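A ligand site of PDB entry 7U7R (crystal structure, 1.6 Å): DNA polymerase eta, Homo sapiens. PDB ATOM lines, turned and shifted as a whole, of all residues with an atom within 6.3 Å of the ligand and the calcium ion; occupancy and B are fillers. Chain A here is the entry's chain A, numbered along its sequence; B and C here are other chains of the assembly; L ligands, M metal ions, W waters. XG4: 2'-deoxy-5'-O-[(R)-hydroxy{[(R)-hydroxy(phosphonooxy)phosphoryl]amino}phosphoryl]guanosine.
Water W3 bridges OD2 of Asp 16 and O2G of the ligand. Water W6 lies within hydrogen-bond range of O2B of the ligand (2.6 Å), NH2 of Arg 58 (2.7 Å) and N of Val 53 (2.9 Å). Water W5 lies within hydrogen-bond range of the backbone carbonyl oxygen of Ile 51 (2.9 Å) and a nitrogen (N3A) of the ligand (2.9 Å). Water W1 bridges the side-chain hydroxyl of Ser 116 (3.1 Å) and an oxygen (O5') of the ligand (3.3 Å).
Within 4 Å of the calcium ion: Asp 16, Met 17 and Asp 118. The nearest printed residue that does not touch the calcium ion is Lys 234 (4.1 Å).
O of Met 17 sits close to NZ of Lys 234. The backbone NH (N) of Asp 16 lies within hydrogen-bond range of the backbone carbonyl oxygen (O) of Ser 216. N1 of DT 8 of chain B is in hydrogen-bond range of NH2 of Arg 64. O4 of DT 4 of chain C is in hydrogen-bond range of the guanidinium group (NH2) of Arg 64, at 3.2 Å. The side-chain hydroxyl of Tyr 55 is in hydrogen-bond range of the guanidinium group of Arg 58 (3.1 Å). The guanidinium group of Arg 64 lies within hydrogen-bond range of the side-chain hydroxyl of Ser 65 (3.1 Å). OD1 of Asp 18 is in salt-bridge range of NZ of Lys 234 (2.8 Å). OG of Ser 216 sits at hydrogen-bond distance from OD1 of Asp 18, 2.8 Å away.
The calcium ion is bound by the backbone carbonyl oxygen of Met 17 (2.2 Å), an oxygen (O3G) of the ligand (2.3 Å), the side-chain carboxylate of Asp 16 (2.3 Å), an oxygen (O1B) of the ligand (2.3 Å), the side-chain carboxylate of Asp 118 (2.3 Å) and an oxygen (O1A) of the ligand (2.5 Å). The calcium ion has six donor atoms within binding distance.
O3' of DT 8 of chain B lies close to an oxygen (O2A) of the ligand (2.4 Å). N1 of the ligand lies within hydrogen-bond range of O2 of DT 4 of chain C (2.5 Å). The side-chain hydroxyl of Tyr 55 sits at hydrogen-bond distance from an oxygen (O1G) of the ligand (2.7 Å). O1G of the ligand is in hydrogen-bond range of N of Cys 19, 2.8 Å away. The guanidinium group of Arg 58 is in salt-bridge range of an oxygen (O2G) of the ligand (3.2 Å). The backbone NH (N) of Phe 21 is in hydrogen-bond range of an oxygen (O3') of the ligand (3.0 Å). The backbone NH of Phe 20 is in hydrogen-bond range of an oxygen (O3') of the ligand (3.4 Å). O6 of the ligand is in hydrogen-bond range of NH2 of Arg 64 (3.1 Å). The side-chain amino group (NZ) of Lys 234 is in salt-bridge range of an oxygen (O1G) of the ligand, 3.2 Å away. O4' of DA 5 of chain C sits at hydrogen-bond distance from N2 of the ligand. N3 of DA 5 of chain C is in hydrogen-bond range of N1 of the ligand, at 3.2 Å.
Merely in contact with the ligand: Asp 18, Ile 51, Ala 52, Gln 41, Ile 117 and Leu 92. Hydrophobic or aromatic side chains that line the ligand: Phe 20, Phe 21, Ile 51, Ala 52, Tyr 55, Leu 92 and Ile 117. The nearest printed residue that does not touch the ligand is Val 53 (4.7 Å).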
ATOM      1  N   ASP A  16     -34.663   4.113  21.912  1.00  0.00           N
ATOM      2  CA  ASP A  16     -33.522   3.227  22.163  1.00  0.00           C
ATOM      3  C   ASP A  16     -32.344   3.675  21.298  1.00  0.00           C
ATOM      4  O   ASP A  16     -32.448   3.704  20.074  1.00  0.00           O
ATOM      5  CB  ASP A  16     -33.926   1.784  21.849  1.00  0.00           C
ATOM      6  CG  ASP A  16     -32.891   0.776  22.269  1.00  0.00           C
ATOM      7  OD1 ASP A  16     -31.891   1.178  22.893  1.00  0.00           O
ATOM      8  OD2 ASP A  16     -33.132  -0.433  22.029  1.00  0.00           O
ATOM      9  N   MET A  17     -31.207   3.965  21.937  1.00  0.00           N
ATOM     10  CA  MET A  17     -30.082   4.419  21.120  1.00  0.00           C
ATOM     11  C   MET A  17     -29.553   3.261  20.277  1.00  0.00           C
ATOM     12  O   MET A  17     -29.477   2.137  20.761  1.00  0.00           O
ATOM     13  CB  MET A  17     -28.975   5.000  22.027  1.00  0.00           C
ATOM     14  CG  MET A  17     -29.499   5.973  23.054  1.00  0.00           C
ATOM     15  SD  MET A  17     -30.198   7.444  22.254  1.00  0.00           S
ATOM     16  CE  MET A  17     -28.838   7.942  21.259  1.00  0.00           C
ATOM     17  N   ASP A  18     -29.243   3.513  19.023  1.00  0.00           N
ATOM     18  CA  ASP A  18     -28.673   2.431  18.178  1.00  0.00           C
ATOM     19  C   ASP A  18     -27.245   2.111  18.637  1.00  0.00           C
ATOM     20  O   ASP A  18     -26.514   3.075  18.858  1.00  0.00           O
ATOM     21  CB  ASP A  18     -28.670   2.833  16.710  1.00  0.00           C
ATOM     22  CG  ASP A  18     -30.047   3.184  16.165  1.00  0.00           C
ATOM     23  OD1 ASP A  18     -31.019   2.570  16.614  1.00  0.00           O
ATOM     24  OD2 ASP A  18     -30.119   4.058  15.292  1.00  0.00           O
ATOM     25  N   CYS A  19     -26.881   0.831  18.682  1.00  0.00           N
ATOM     26  CA  CYS A  19     -25.504   0.381  19.035  1.00  0.00           C
ATOM     27  C   CYS A  19     -24.834   1.429  19.933  1.00  0.00           C
ATOM     28  O   CYS A  19     -23.773   1.908  19.563  1.00  0.00           O
ATOM     29  CB  CYS A  19     -24.719   0.016  17.775  1.00  0.00           C
ATOM     30  SG  CYS A  19     -24.672   1.250  16.459  1.00  0.00           S
ATOM     31  N   PHE A  20     -25.398   1.690  21.113  1.00  0.00           N
ATOM     32  CA  PHE A  20     -24.970   2.845  21.951  1.00  0.00           C
ATOM     33  C   PHE A  20     -23.462   2.942  22.216  1.00  0.00           C
ATOM     34  O   PHE A  20     -22.878   3.940  21.816  1.00  0.00           O
ATOM     35  CB  PHE A  20     -25.740   2.902  23.273  1.00  0.00           C
ATOM     36  CG  PHE A  20     -25.535   4.190  24.031  1.00  0.00           C
ATOM     37  CD1 PHE A  20     -25.627   5.414  23.385  1.00  0.00           C
ATOM     38  CD2 PHE A  20     -25.237   4.190  25.383  1.00  0.00           C
ATOM     39  CE1 PHE A  20     -25.428   6.602  24.066  1.00  0.00           C
ATOM     40  CE2 PHE A  20     -25.040   5.385  26.070  1.00  0.00           C
ATOM     41  CZ  PHE A  20     -25.136   6.591  25.412  1.00  0.00           C
ATOM     42  N   PHE A  21     -22.887   1.953  22.888  1.00  0.00           N
ATOM     43  CA  PHE A  21     -21.448   2.080  23.245  1.00  0.00           C
ATOM     44  C   PHE A  21     -20.622   2.306  21.968  1.00  0.00           C
ATOM     45  O   PHE A  21     -19.662   3.057  22.016  1.00  0.00           O
ATOM     46  CB  PHE A  21     -20.978   0.867  24.057  1.00  0.00           C
ATOM     47  CG  PHE A  21     -21.448   0.784  25.494  1.00  0.00           C
ATOM     48  CD1 PHE A  21     -22.591   1.429  25.916  1.00  0.00           C
ATOM     49  CD2 PHE A  21     -20.752   0.026  26.416  1.00  0.00           C
ATOM     50  CE1 PHE A  21     -23.026   1.329  27.222  1.00  0.00           C
ATOM     51  CE2 PHE A  21     -21.176  -0.068  27.734  1.00  0.00           C
ATOM     52  CZ  PHE A  21     -22.315   0.586  28.134  1.00  0.00           C
ATOM     53  N   VAL A  22     -20.999   1.653  20.870  1.00  0.00           N
ATOM     54  CA  VAL A  22     -20.286   1.853  19.578  1.00  0.00           C
ATOM     55  C   VAL A  22     -20.397   3.333  19.151  1.00  0.00           C
ATOM     56  O   VAL A  22     -19.385   3.921  18.814  1.00  0.00           O
ATOM     57  CB  VAL A  22     -20.812   0.913  18.479  1.00  0.00           C
ATOM     58  CG1 VAL A  22     -20.402   1.378  17.093  1.00  0.00           C
ATOM     59  CG2 VAL A  22     -20.372  -0.516  18.712  1.00  0.00           C
ATOM     60  N   GLN A  41     -15.101  -5.727  26.228  1.00  0.00           N
ATOM     61  CA  GLN A  41     -14.492  -5.548  27.542  1.00  0.00           C
ATOM     62  C   GLN A  41     -13.415  -6.602  27.776  1.00  0.00           C
ATOM     63  O   GLN A  41     -13.623  -7.795  27.502  1.00  0.00           O
ATOM     64  CB  GLN A  41     -15.540  -5.459  28.677  1.00  0.00           C
ATOM     65  CG  GLN A  41     -16.686  -6.382  28.703  1.00  0.00           C
ATOM     66  CD  GLN A  41     -17.848  -5.881  29.607  1.00  0.00           C
ATOM     67  OE1 GLN A  41     -17.895  -4.724  30.101  1.00  0.00           O
ATOM     68  NE2 GLN A  41     -18.754  -6.774  29.848  1.00  0.00           N
ATOM     69  N   ILE A  51     -19.709  -6.489  23.535  1.00  0.00           N
ATOM     70  CA  ILE A  51     -20.980  -6.080  24.129  1.00  0.00           C
ATOM     71  C   ILE A  51     -21.793  -5.118  23.269  1.00  0.00           C
ATOM     72  O   ILE A  51     -22.950  -4.846  23.618  1.00  0.00           O
ATOM     73  CB  ILE A  51     -20.787  -5.490  25.543  1.00  0.00           C
ATOM     74  CG1 ILE A  51     -19.770  -4.347  25.543  1.00  0.00           C
ATOM     75  CG2 ILE A  51     -20.425  -6.588  26.565  1.00  0.00           C
ATOM     76  CD1 ILE A  51     -19.697  -3.591  26.851  1.00  0.00           C
ATOM     77  N   ALA A  52     -21.268  -4.630  22.147  1.00  0.00           N
ATOM     78  CA  ALA A  52     -22.023  -3.743  21.266  1.00  0.00           C
ATOM     79  C   ALA A  52     -21.423  -3.839  19.878  1.00  0.00           C
ATOM     80  O   ALA A  52     -20.199  -4.003  19.749  1.00  0.00           O
ATOM     81  CB  ALA A  52     -22.016  -2.290  21.762  1.00  0.00           C
ATOM     82  N   VAL A  53     -22.262  -3.732  18.838  1.00  0.00           N
ATOM     83  CA  VAL A  53     -21.871  -4.060  17.460  1.00  0.00           C
ATOM     84  C   VAL A  53     -22.531  -3.071  16.497  1.00  0.00           C
ATOM     85  O   VAL A  53     -23.761  -2.961  16.473  1.00  0.00           O
ATOM     86  CB  VAL A  53     -22.316  -5.484  17.085  1.00  0.00           C
ATOM     87  CG1 VAL A  53     -21.774  -5.862  15.723  1.00  0.00           C
ATOM     88  CG2 VAL A  53     -21.839  -6.469  18.123  1.00  0.00           C
ATOM     89  N   TYR A  55     -23.970  -1.650  12.919  1.00  0.00           N
ATOM     90  CA  TYR A  55     -24.823  -2.388  11.982  1.00  0.00           C
ATOM     91  C   TYR A  55     -24.015  -2.914  10.789  1.00  0.00           C
ATOM     92  O   TYR A  55     -24.286  -4.024  10.281  1.00  0.00           O
ATOM     93  CB  TYR A  55     -25.997  -1.481  11.570  1.00  0.00           C
ATOM     94  CG  TYR A  55     -27.059  -1.464  12.668  1.00  0.00           C
ATOM     95  CD1 TYR A  55     -26.869  -0.715  13.822  1.00  0.00           C
ATOM     96  CD2 TYR A  55     -28.198  -2.250  12.591  1.00  0.00           C
ATOM     97  CE1 TYR A  55     -27.813  -0.726  14.861  1.00  0.00           C
ATOM     98  CE2 TYR A  55     -29.154  -2.261  13.624  1.00  0.00           C
ATOM     99  CZ  TYR A  55     -28.945  -1.510  14.754  1.00  0.00           C
ATOM    100  OH  TYR A  55     -29.871  -1.513  15.790  1.00  0.00           O
ATOM    101  N   ARG A  58     -22.743  -6.081  12.147  1.00  0.00           N
ATOM    102  CA  ARG A  58     -23.827  -7.058  12.262  1.00  0.00           C
ATOM    103  C   ARG A  58     -24.073  -7.767  10.933  1.00  0.00           C
ATOM    104  O   ARG A  58     -24.445  -8.943  10.918  1.00  0.00           O
ATOM    105  CB  ARG A  58     -25.112  -6.380  12.747  1.00  0.00           C
ATOM    106  CG  ARG A  58     -25.027  -5.806  14.137  1.00  0.00           C
ATOM    107  CD  ARG A  58     -26.327  -5.161  14.561  1.00  0.00           C
ATOM    108  NE  ARG A  58     -26.162  -4.407  15.788  1.00  0.00           N
ATOM    109  CZ  ARG A  58     -27.160  -4.000  16.568  1.00  0.00           C
ATOM    110  NH1 ARG A  58     -28.416  -4.256  16.245  1.00  0.00           N
ATOM    111  NH2 ARG A  58     -26.880  -3.309  17.667  1.00  0.00           N
ATOM    112  N   ARG A  64     -23.312  -9.357  20.015  1.00  0.00           N
ATOM    113  CA  ARG A  64     -23.073  -9.307  21.441  1.00  0.00           C
ATOM    114  C   ARG A  64     -22.797 -10.701  21.987  1.00  0.00           C
ATOM    115  O   ARG A  64     -23.305 -11.701  21.461  1.00  0.00           O
ATOM    116  CB  ARG A  64     -24.299  -8.660  22.078  1.00  0.00           C
ATOM    117  CG  ARG A  64     -24.314  -8.586  23.549  1.00  0.00           C
ATOM    118  CD  ARG A  64     -25.738  -8.421  24.026  1.00  0.00           C
ATOM    119  NE  ARG A  64     -25.733  -8.551  25.474  1.00  0.00           N
ATOM    120  CZ  ARG A  64     -26.045  -9.669  26.104  1.00  0.00           C
ATOM    121  NH1 ARG A  64     -26.521 -10.719  25.464  1.00  0.00           N
ATOM    122  NH2 ARG A  64     -25.855  -9.732  27.422  1.00  0.00           N
ATOM    123  N   SER A  65     -21.968 -10.788  23.034  1.00  0.00           N
ATOM    124  CA  SER A  65     -21.602 -12.000  23.750  1.00  0.00           C
ATOM    125  C   SER A  65     -20.583 -12.832  22.977  1.00  0.00           C
ATOM    126  O   SER A  65     -20.177 -13.869  23.477  1.00  0.00           O
ATOM    127  CB  SER A  65     -22.810 -12.902  24.052  1.00  0.00           C
ATOM    128  OG  SER A  65     -23.857 -12.119  24.604  1.00  0.00           O
ATOM    129  N   LEU A  92     -17.467   1.766  33.267  1.00  0.00           N
ATOM    130  CA  LEU A  92     -18.423   2.202  32.238  1.00  0.00           C
ATOM    131  C   LEU A  92     -18.824   3.672  32.369  1.00  0.00           C
ATOM    132  O   LEU A  92     -19.872   4.071  31.850  1.00  0.00           O
ATOM    133  CB  LEU A  92     -19.656   1.315  32.255  1.00  0.00           C
ATOM    134  CG  LEU A  92     -19.394  -0.192  32.212  1.00  0.00           C
ATOM    135  CD1 LEU A  92     -20.671  -0.988  32.399  1.00  0.00           C
ATOM    136  CD2 LEU A  92     -18.689  -0.582  30.934  1.00  0.00           C
ATOM    137  N   SER A 116     -33.087   1.591  30.754  1.00  0.00           N
ATOM    138  CA  SER A 116     -31.733   1.052  30.781  1.00  0.00           C
ATOM    139  C   SER A 116     -30.793   2.182  30.420  1.00  0.00           C
ATOM    140  O   SER A 116     -31.236   3.299  30.103  1.00  0.00           O
ATOM    141  CB  SER A 116     -31.584  -0.141  29.823  1.00  0.00           C
ATOM    142  OG  SER A 116     -31.390   0.297  28.489  1.00  0.00           O
ATOM    143  N   ILE A 117     -29.488   1.895  30.427  1.00  0.00           N
ATOM    144  CA  ILE A 117     -28.489   2.912  30.082  1.00  0.00           C
ATOM    145  C   ILE A 117     -28.810   3.646  28.781  1.00  0.00           C
ATOM    146  O   ILE A 117     -28.435   4.812  28.619  1.00  0.00           O
ATOM    147  CB  ILE A 117     -27.084   2.287  30.009  1.00  0.00           C
ATOM    148  CG1 ILE A 117     -26.039   3.398  30.095  1.00  0.00           C
ATOM    149  CG2 ILE A 117     -26.892   1.442  28.752  1.00  0.00           C
ATOM    150  CD1 ILE A 117     -24.673   2.887  30.475  1.00  0.00           C
ATOM    151  N   ASP A 118     -29.486   3.004  27.841  1.00  0.00           N
ATOM    152  CA  ASP A 118     -29.676   3.765  26.603  1.00  0.00           C
ATOM    153  C   ASP A 118     -31.104   3.688  26.100  1.00  0.00           C
ATOM    154  O   ASP A 118     -31.372   3.944  24.913  1.00  0.00           O
ATOM    155  CB  ASP A 118     -28.713   3.318  25.516  1.00  0.00           C
ATOM    156  CG  ASP A 118     -29.141   2.040  24.887  1.00  0.00           C
ATOM    157  OD1 ASP A 118     -29.731   1.179  25.585  1.00  0.00           O
ATOM    158  OD2 ASP A 118     -28.914   1.903  23.669  1.00  0.00           O
ATOM    159  N   GLU A 119     -32.048   3.437  26.999  1.00  0.00           N
ATOM    160  CA  GLU A 119     -33.406   3.466  26.488  1.00  0.00           C
ATOM    161  C   GLU A 119     -34.333   3.993  27.551  1.00  0.00           C
ATOM    162  O   GLU A 119     -34.130   3.784  28.756  1.00  0.00           O
ATOM    163  CB  GLU A 119     -33.869   2.093  25.997  1.00  0.00           C
ATOM    164  CG  GLU A 119     -34.382   1.206  27.067  1.00  0.00           C
ATOM    165  CD  GLU A 119     -34.605  -0.212  26.604  1.00  0.00           C
ATOM    166  OE1 GLU A 119     -33.658  -0.860  26.146  1.00  0.00           O
ATOM    167  OE2 GLU A 119     -35.751  -0.674  26.669  1.00  0.00           O
ATOM    168  N   SER A 216     -33.511   4.715  17.498  1.00  0.00           N
ATOM    169  CA  SER A 216     -34.761   4.228  16.955  1.00  0.00           C
ATOM    170  C   SER A 216     -35.839   4.466  18.004  1.00  0.00           C
ATOM    171  O   SER A 216     -35.537   4.701  19.168  1.00  0.00           O
ATOM    172  CB  SER A 216     -34.653   2.741  16.606  1.00  0.00           C
ATOM    173  OG  SER A 216     -33.660   2.533  15.613  1.00  0.00           O
ATOM    174  N   LYS A 227     -42.128  -0.828  22.733  1.00  0.00           N
ATOM    175  CA  LYS A 227     -40.829  -1.506  22.675  1.00  0.00           C
ATOM    176  C   LYS A 227     -40.760  -2.412  21.449  1.00  0.00           C
ATOM    177  O   LYS A 227     -39.770  -2.396  20.683  1.00  0.00           O
ATOM    178  CB  LYS A 227     -40.634  -2.311  23.958  1.00  0.00           C
ATOM    179  CG  LYS A 227     -39.369  -3.178  24.031  1.00  0.00           C
ATOM    180  CD  LYS A 227     -38.129  -2.320  23.957  1.00  0.00           C
ATOM    181  CE  LYS A 227     -36.859  -3.150  24.198  1.00  0.00           C
ATOM    182  NZ  LYS A 227     -35.620  -2.325  24.084  1.00  0.00           N
ATOM    183  N   LYS A 234     -35.036  -0.873  12.907  1.00  0.00           N
ATOM    184  CA  LYS A 234     -33.757  -0.327  13.300  1.00  0.00           C
ATOM    185  C   LYS A 234     -32.765  -0.444  12.144  1.00  0.00           C
ATOM    186  O   LYS A 234     -32.859  -1.360  11.334  1.00  0.00           O
ATOM    187  CB  LYS A 234     -33.236  -1.104  14.512  1.00  0.00           C
ATOM    188  CG  LYS A 234     -33.707  -0.572  15.877  1.00  0.00           C
ATOM    189  CD  LYS A 234     -32.827  -1.067  17.039  1.00  0.00           C
ATOM    190  CE  LYS A 234     -32.978  -0.171  18.289  1.00  0.00           C
ATOM    191  NZ  LYS A 234     -31.805   0.764  18.581  1.00  0.00           N
ATOM    192  N   PRO A 235     -31.771   0.473  12.056  1.00  0.00           N
ATOM    193  CA  PRO A 235     -31.471   1.620  12.915  1.00  0.00           C
ATOM    194  C   PRO A 235     -32.018   2.934  12.395  1.00  0.00           C
ATOM    195  O   PRO A 235     -32.430   3.031  11.226  1.00  0.00           O
ATOM    196  CB  PRO A 235     -29.939   1.660  12.897  1.00  0.00           C
ATOM    197  CG  PRO A 235     -29.625   1.286  11.451  1.00  0.00           C
ATOM    198  CD  PRO A 235     -30.687   0.263  11.069  1.00  0.00           C
ATOM    199  P    DT B   8     -33.385  -7.851  25.764  1.00  0.00           P
ATOM    200  OP1  DT B   8     -34.455  -7.544  24.749  1.00  0.00           O
ATOM    201  OP2  DT B   8     -32.688  -9.199  25.530  1.00  0.00           O
ATOM    202  O5'  DT B   8     -32.266  -6.700  25.547  1.00  0.00           O
ATOM    203  C5'  DT B   8     -31.747  -5.960  26.682  1.00  0.00           C
ATOM    204  C4'  DT B   8     -30.234  -5.947  26.597  1.00  0.00           C
ATOM    205  O4'  DT B   8     -29.690  -6.522  27.807  1.00  0.00           O
ATOM    206  C3'  DT B   8     -29.654  -6.752  25.439  1.00  0.00           C
ATOM    207  O3'  DT B   8     -28.506  -6.148  24.844  1.00  0.00           O
ATOM    208  C2'  DT B   8     -29.184  -8.023  26.120  1.00  0.00           C
ATOM    209  C1'  DT B   8     -28.692  -7.452  27.427  1.00  0.00           C
ATOM    210  N1   DT B   8     -28.501  -8.445  28.488  1.00  0.00           N
ATOM    211  C2   DT B   8     -27.754  -8.082  29.583  1.00  0.00           C
ATOM    212  O2   DT B   8     -27.318  -6.951  29.737  1.00  0.00           O
ATOM    213  N3   DT B   8     -27.566  -9.087  30.496  1.00  0.00           N
ATOM    214  C4   DT B   8     -28.013 -10.381  30.411  1.00  0.00           C
ATOM    215  O4   DT B   8     -27.775 -11.171  31.318  1.00  0.00           O
ATOM    216  C5   DT B   8     -28.773 -10.697  29.222  1.00  0.00           C
ATOM    217  C7   DT B   8     -29.309 -12.084  29.053  1.00  0.00           C
ATOM    218  C6   DT B   8     -28.965  -9.725  28.326  1.00  0.00           C
ATOM    219  P    DT C   4     -18.015 -14.268  31.185  1.00  0.00           P
ATOM    220  OP1  DT C   4     -16.720 -14.935  30.970  1.00  0.00           O
ATOM    221  OP2  DT C   4     -19.085 -14.901  31.995  1.00  0.00           O
ATOM    222  O5'  DT C   4     -17.665 -12.839  31.797  1.00  0.00           O
ATOM    223  C5'  DT C   4     -16.980 -11.861  30.989  1.00  0.00           C
ATOM    224  C4'  DT C   4     -17.318 -10.456  31.424  1.00  0.00           C
ATOM    225  O4'  DT C   4     -18.539 -10.012  30.785  1.00  0.00           O
ATOM    226  C3'  DT C   4     -17.541 -10.248  32.922  1.00  0.00           C
ATOM    227  O3'  DT C   4     -16.968  -8.974  33.202  1.00  0.00           O
ATOM    228  C2'  DT C   4     -19.053 -10.252  33.057  1.00  0.00           C
ATOM    229  C1'  DT C   4     -19.491  -9.617  31.768  1.00  0.00           C
ATOM    230  N1   DT C   4     -20.805 -10.048  31.292  1.00  0.00           N
ATOM    231  C2   DT C   4     -21.561  -9.158  30.581  1.00  0.00           C
ATOM    232  O2   DT C   4     -21.219  -8.009  30.366  1.00  0.00           O
ATOM    233  N3   DT C   4     -22.759  -9.656  30.140  1.00  0.00           N
ATOM    234  C4   DT C   4     -23.257 -10.932  30.323  1.00  0.00           C
ATOM    235  O4   DT C   4     -24.350 -11.235  29.873  1.00  0.00           O
ATOM    236  C5   DT C   4     -22.394 -11.822  31.073  1.00  0.00           C
ATOM    237  C7   DT C   4     -22.850 -13.225  31.339  1.00  0.00           C
ATOM    238  C6   DT C   4     -21.224 -11.338  31.503  1.00  0.00           C
ATOM    239  P    DA C   5     -16.946  -8.326  34.729  1.00  0.00           P
ATOM    240  OP1  DA C   5     -15.605  -7.783  34.988  1.00  0.00           O
ATOM    241  OP2  DA C   5     -17.547  -9.267  35.705  1.00  0.00           O
ATOM    242  O5'  DA C   5     -17.972  -7.110  34.629  1.00  0.00           O
ATOM    243  C5'  DA C   5     -17.871  -6.105  33.615  1.00  0.00           C
ATOM    244  C4'  DA C   5     -19.009  -5.123  33.735  1.00  0.00           C
ATOM    245  O4'  DA C   5     -20.219  -5.731  33.211  1.00  0.00           O
ATOM    246  C3'  DA C   5     -19.335  -4.683  35.170  1.00  0.00           C
ATOM    247  O3'  DA C   5     -19.591  -3.269  35.162  1.00  0.00           O
ATOM    248  C2'  DA C   5     -20.554  -5.526  35.525  1.00  0.00           C
ATOM    249  C1'  DA C   5     -21.248  -5.700  34.191  1.00  0.00           C
ATOM    250  N9   DA C   5     -22.009  -6.938  34.071  1.00  0.00           N
ATOM    251  C8   DA C   5     -21.742  -8.147  34.648  1.00  0.00           C
ATOM    252  N7   DA C   5     -22.609  -9.086  34.353  1.00  0.00           N
ATOM    253  C5   DA C   5     -23.518  -8.441  33.526  1.00  0.00           C
ATOM    254  C6   DA C   5     -24.676  -8.876  32.863  1.00  0.00           C
ATOM    255  N6   DA C   5     -25.143 -10.129  32.948  1.00  0.00           N
ATOM    256  N1   DA C   5     -25.347  -7.992  32.101  1.00  0.00           N
ATOM    257  C2   DA C   5     -24.880  -6.739  32.015  1.00  0.00           C
ATOM    258  N3   DA C   5     -23.797  -6.201  32.593  1.00  0.00           N
ATOM    259  C4   DA C   5     -23.159  -7.117  33.332  1.00  0.00           C
ATOM    260  P    DT C   6     -20.001  -2.461  36.509  1.00  0.00           P
ATOM    261  OP1  DT C   6     -20.192  -1.052  36.138  1.00  0.00           O
ATOM    262  OP2  DT C   6     -19.068  -2.812  37.592  1.00  0.00           O
ATOM    263  O5'  DT C   6     -21.374  -3.110  36.938  1.00  0.00           O
ATOM    264  C5'  DT C   6     -22.488  -2.333  37.312  1.00  0.00           C
ATOM    265  C4'  DT C   6     -23.634  -2.514  36.345  1.00  0.00           C
ATOM    266  O4'  DT C   6     -23.788  -3.881  35.915  1.00  0.00           O
ATOM    267  C3'  DT C   6     -24.954  -2.129  36.988  1.00  0.00           C
ATOM    268  O3'  DT C   6     -25.261  -0.852  36.446  1.00  0.00           O
ATOM    269  C2'  DT C   6     -25.935  -3.183  36.507  1.00  0.00           C
ATOM    270  C1'  DT C   6     -25.138  -4.050  35.559  1.00  0.00           C
ATOM    271  N1   DT C   6     -25.462  -5.485  35.686  1.00  0.00           N
ATOM    272  C2   DT C   6     -26.529  -5.962  34.967  1.00  0.00           C
ATOM    273  O2   DT C   6     -27.205  -5.262  34.225  1.00  0.00           O
ATOM    274  N3   DT C   6     -26.786  -7.298  35.122  1.00  0.00           N
ATOM    275  C4   DT C   6     -26.085  -8.190  35.917  1.00  0.00           C
ATOM    276  O4   DT C   6     -26.416  -9.361  35.969  1.00  0.00           O
ATOM    277  C5   DT C   6     -24.976  -7.613  36.653  1.00  0.00           C
ATOM    278  C7   DT C   6     -24.171  -8.506  37.545  1.00  0.00           C
ATOM    279  C6   DT C   6     -24.735  -6.308  36.509  1.00  0.00           C
HETATM  280  N1  XG4 L   1     -22.617  -6.098  29.593  1.00  0.00           N
HETATM  281  C2  XG4 L   1     -22.318  -4.761  29.583  1.00  0.00           C
HETATM  282  N2  XG4 L   1     -21.402  -4.365  30.473  1.00  0.00           N
HETATM  283  N3  XG4 L   1     -22.842  -3.844  28.768  1.00  0.00           N
HETATM  284  C4  XG4 L   1     -23.750  -4.330  27.940  1.00  0.00           C
HETATM  285  C5  XG4 L   1     -24.144  -5.622  27.843  1.00  0.00           C
HETATM  286  C6  XG4 L   1     -23.539  -6.545  28.721  1.00  0.00           C
HETATM  287  O6  XG4 L   1     -23.850  -7.745  28.737  1.00  0.00           O
HETATM  288  N7  XG4 L   1     -25.122  -5.759  26.863  1.00  0.00           N
HETATM  289  C8  XG4 L   1     -25.267  -4.542  26.379  1.00  0.00           C
HETATM  290  N9  XG4 L   1     -24.454  -3.633  26.988  1.00  0.00           N
HETATM  291  PA  XG4 L   1     -28.607  -2.504  23.909  1.00  0.00           P
HETATM  292  PB  XG4 L   1     -27.250  -1.583  21.482  1.00  0.00           P
HETATM  293  PG  XG4 L   1     -29.263  -1.760  19.393  1.00  0.00           P
HETATM  294  C1' XG4 L   1     -24.266  -2.223  26.678  1.00  0.00           C
HETATM  295  O1A XG4 L   1     -29.678  -1.535  23.646  1.00  0.00           O
HETATM  296  O1B XG4 L   1     -27.628  -0.244  21.955  1.00  0.00           O
HETATM  297  O1G XG4 L   1     -29.110  -0.849  18.245  1.00  0.00           O
HETATM  298  C2' XG4 L   1     -23.711  -1.985  25.279  1.00  0.00           C
HETATM  299  O2A XG4 L   1     -29.254  -3.930  24.260  1.00  0.00           O
HETATM  300  O2B XG4 L   1     -25.711  -1.724  21.269  1.00  0.00           O
HETATM  301  O2G XG4 L   1     -29.773  -3.155  18.966  1.00  0.00           O
HETATM  302  C3' XG4 L   1     -24.901  -1.489  24.483  1.00  0.00           C
HETATM  303  O3' XG4 L   1     -24.450  -0.536  23.529  1.00  0.00           O
HETATM  304  N3A XG4 L   1     -27.658  -2.717  22.586  1.00  0.00           N
HETATM  305  O3B XG4 L   1     -27.856  -2.038  20.094  1.00  0.00           O
HETATM  306  O3G XG4 L   1     -30.146  -1.170  20.512  1.00  0.00           O
HETATM  307  C4' XG4 L   1     -25.759  -0.808  25.550  1.00  0.00           C
HETATM  308  O4' XG4 L   1     -25.543  -1.588  26.743  1.00  0.00           O
HETATM  309  C5' XG4 L   1     -27.239  -0.765  25.258  1.00  0.00           C
HETATM  310  O5' XG4 L   1     -27.741  -2.111  25.161  1.00  0.00           O
HETATM  311 CA    CA M   1     -29.850   0.400  22.139  1.00  0.00          CA
HETATM  312  O   HOH W   1     -30.368  -2.231  27.071  1.00  0.00           O
HETATM  313  O   HOH W   2     -28.904  -5.532  19.605  1.00  0.00           O
HETATM  314  O   HOH W   3     -31.891  -2.805  21.375  1.00  0.00           O
HETATM  315  O   HOH W   4     -27.642  -2.484  28.447  1.00  0.00           O
HETATM  316  O   HOH W   5     -25.733  -4.879  22.838  1.00  0.00           O
HETATM  317  O   HOH W   6     -25.016  -3.604  19.662  1.00  0.00           O
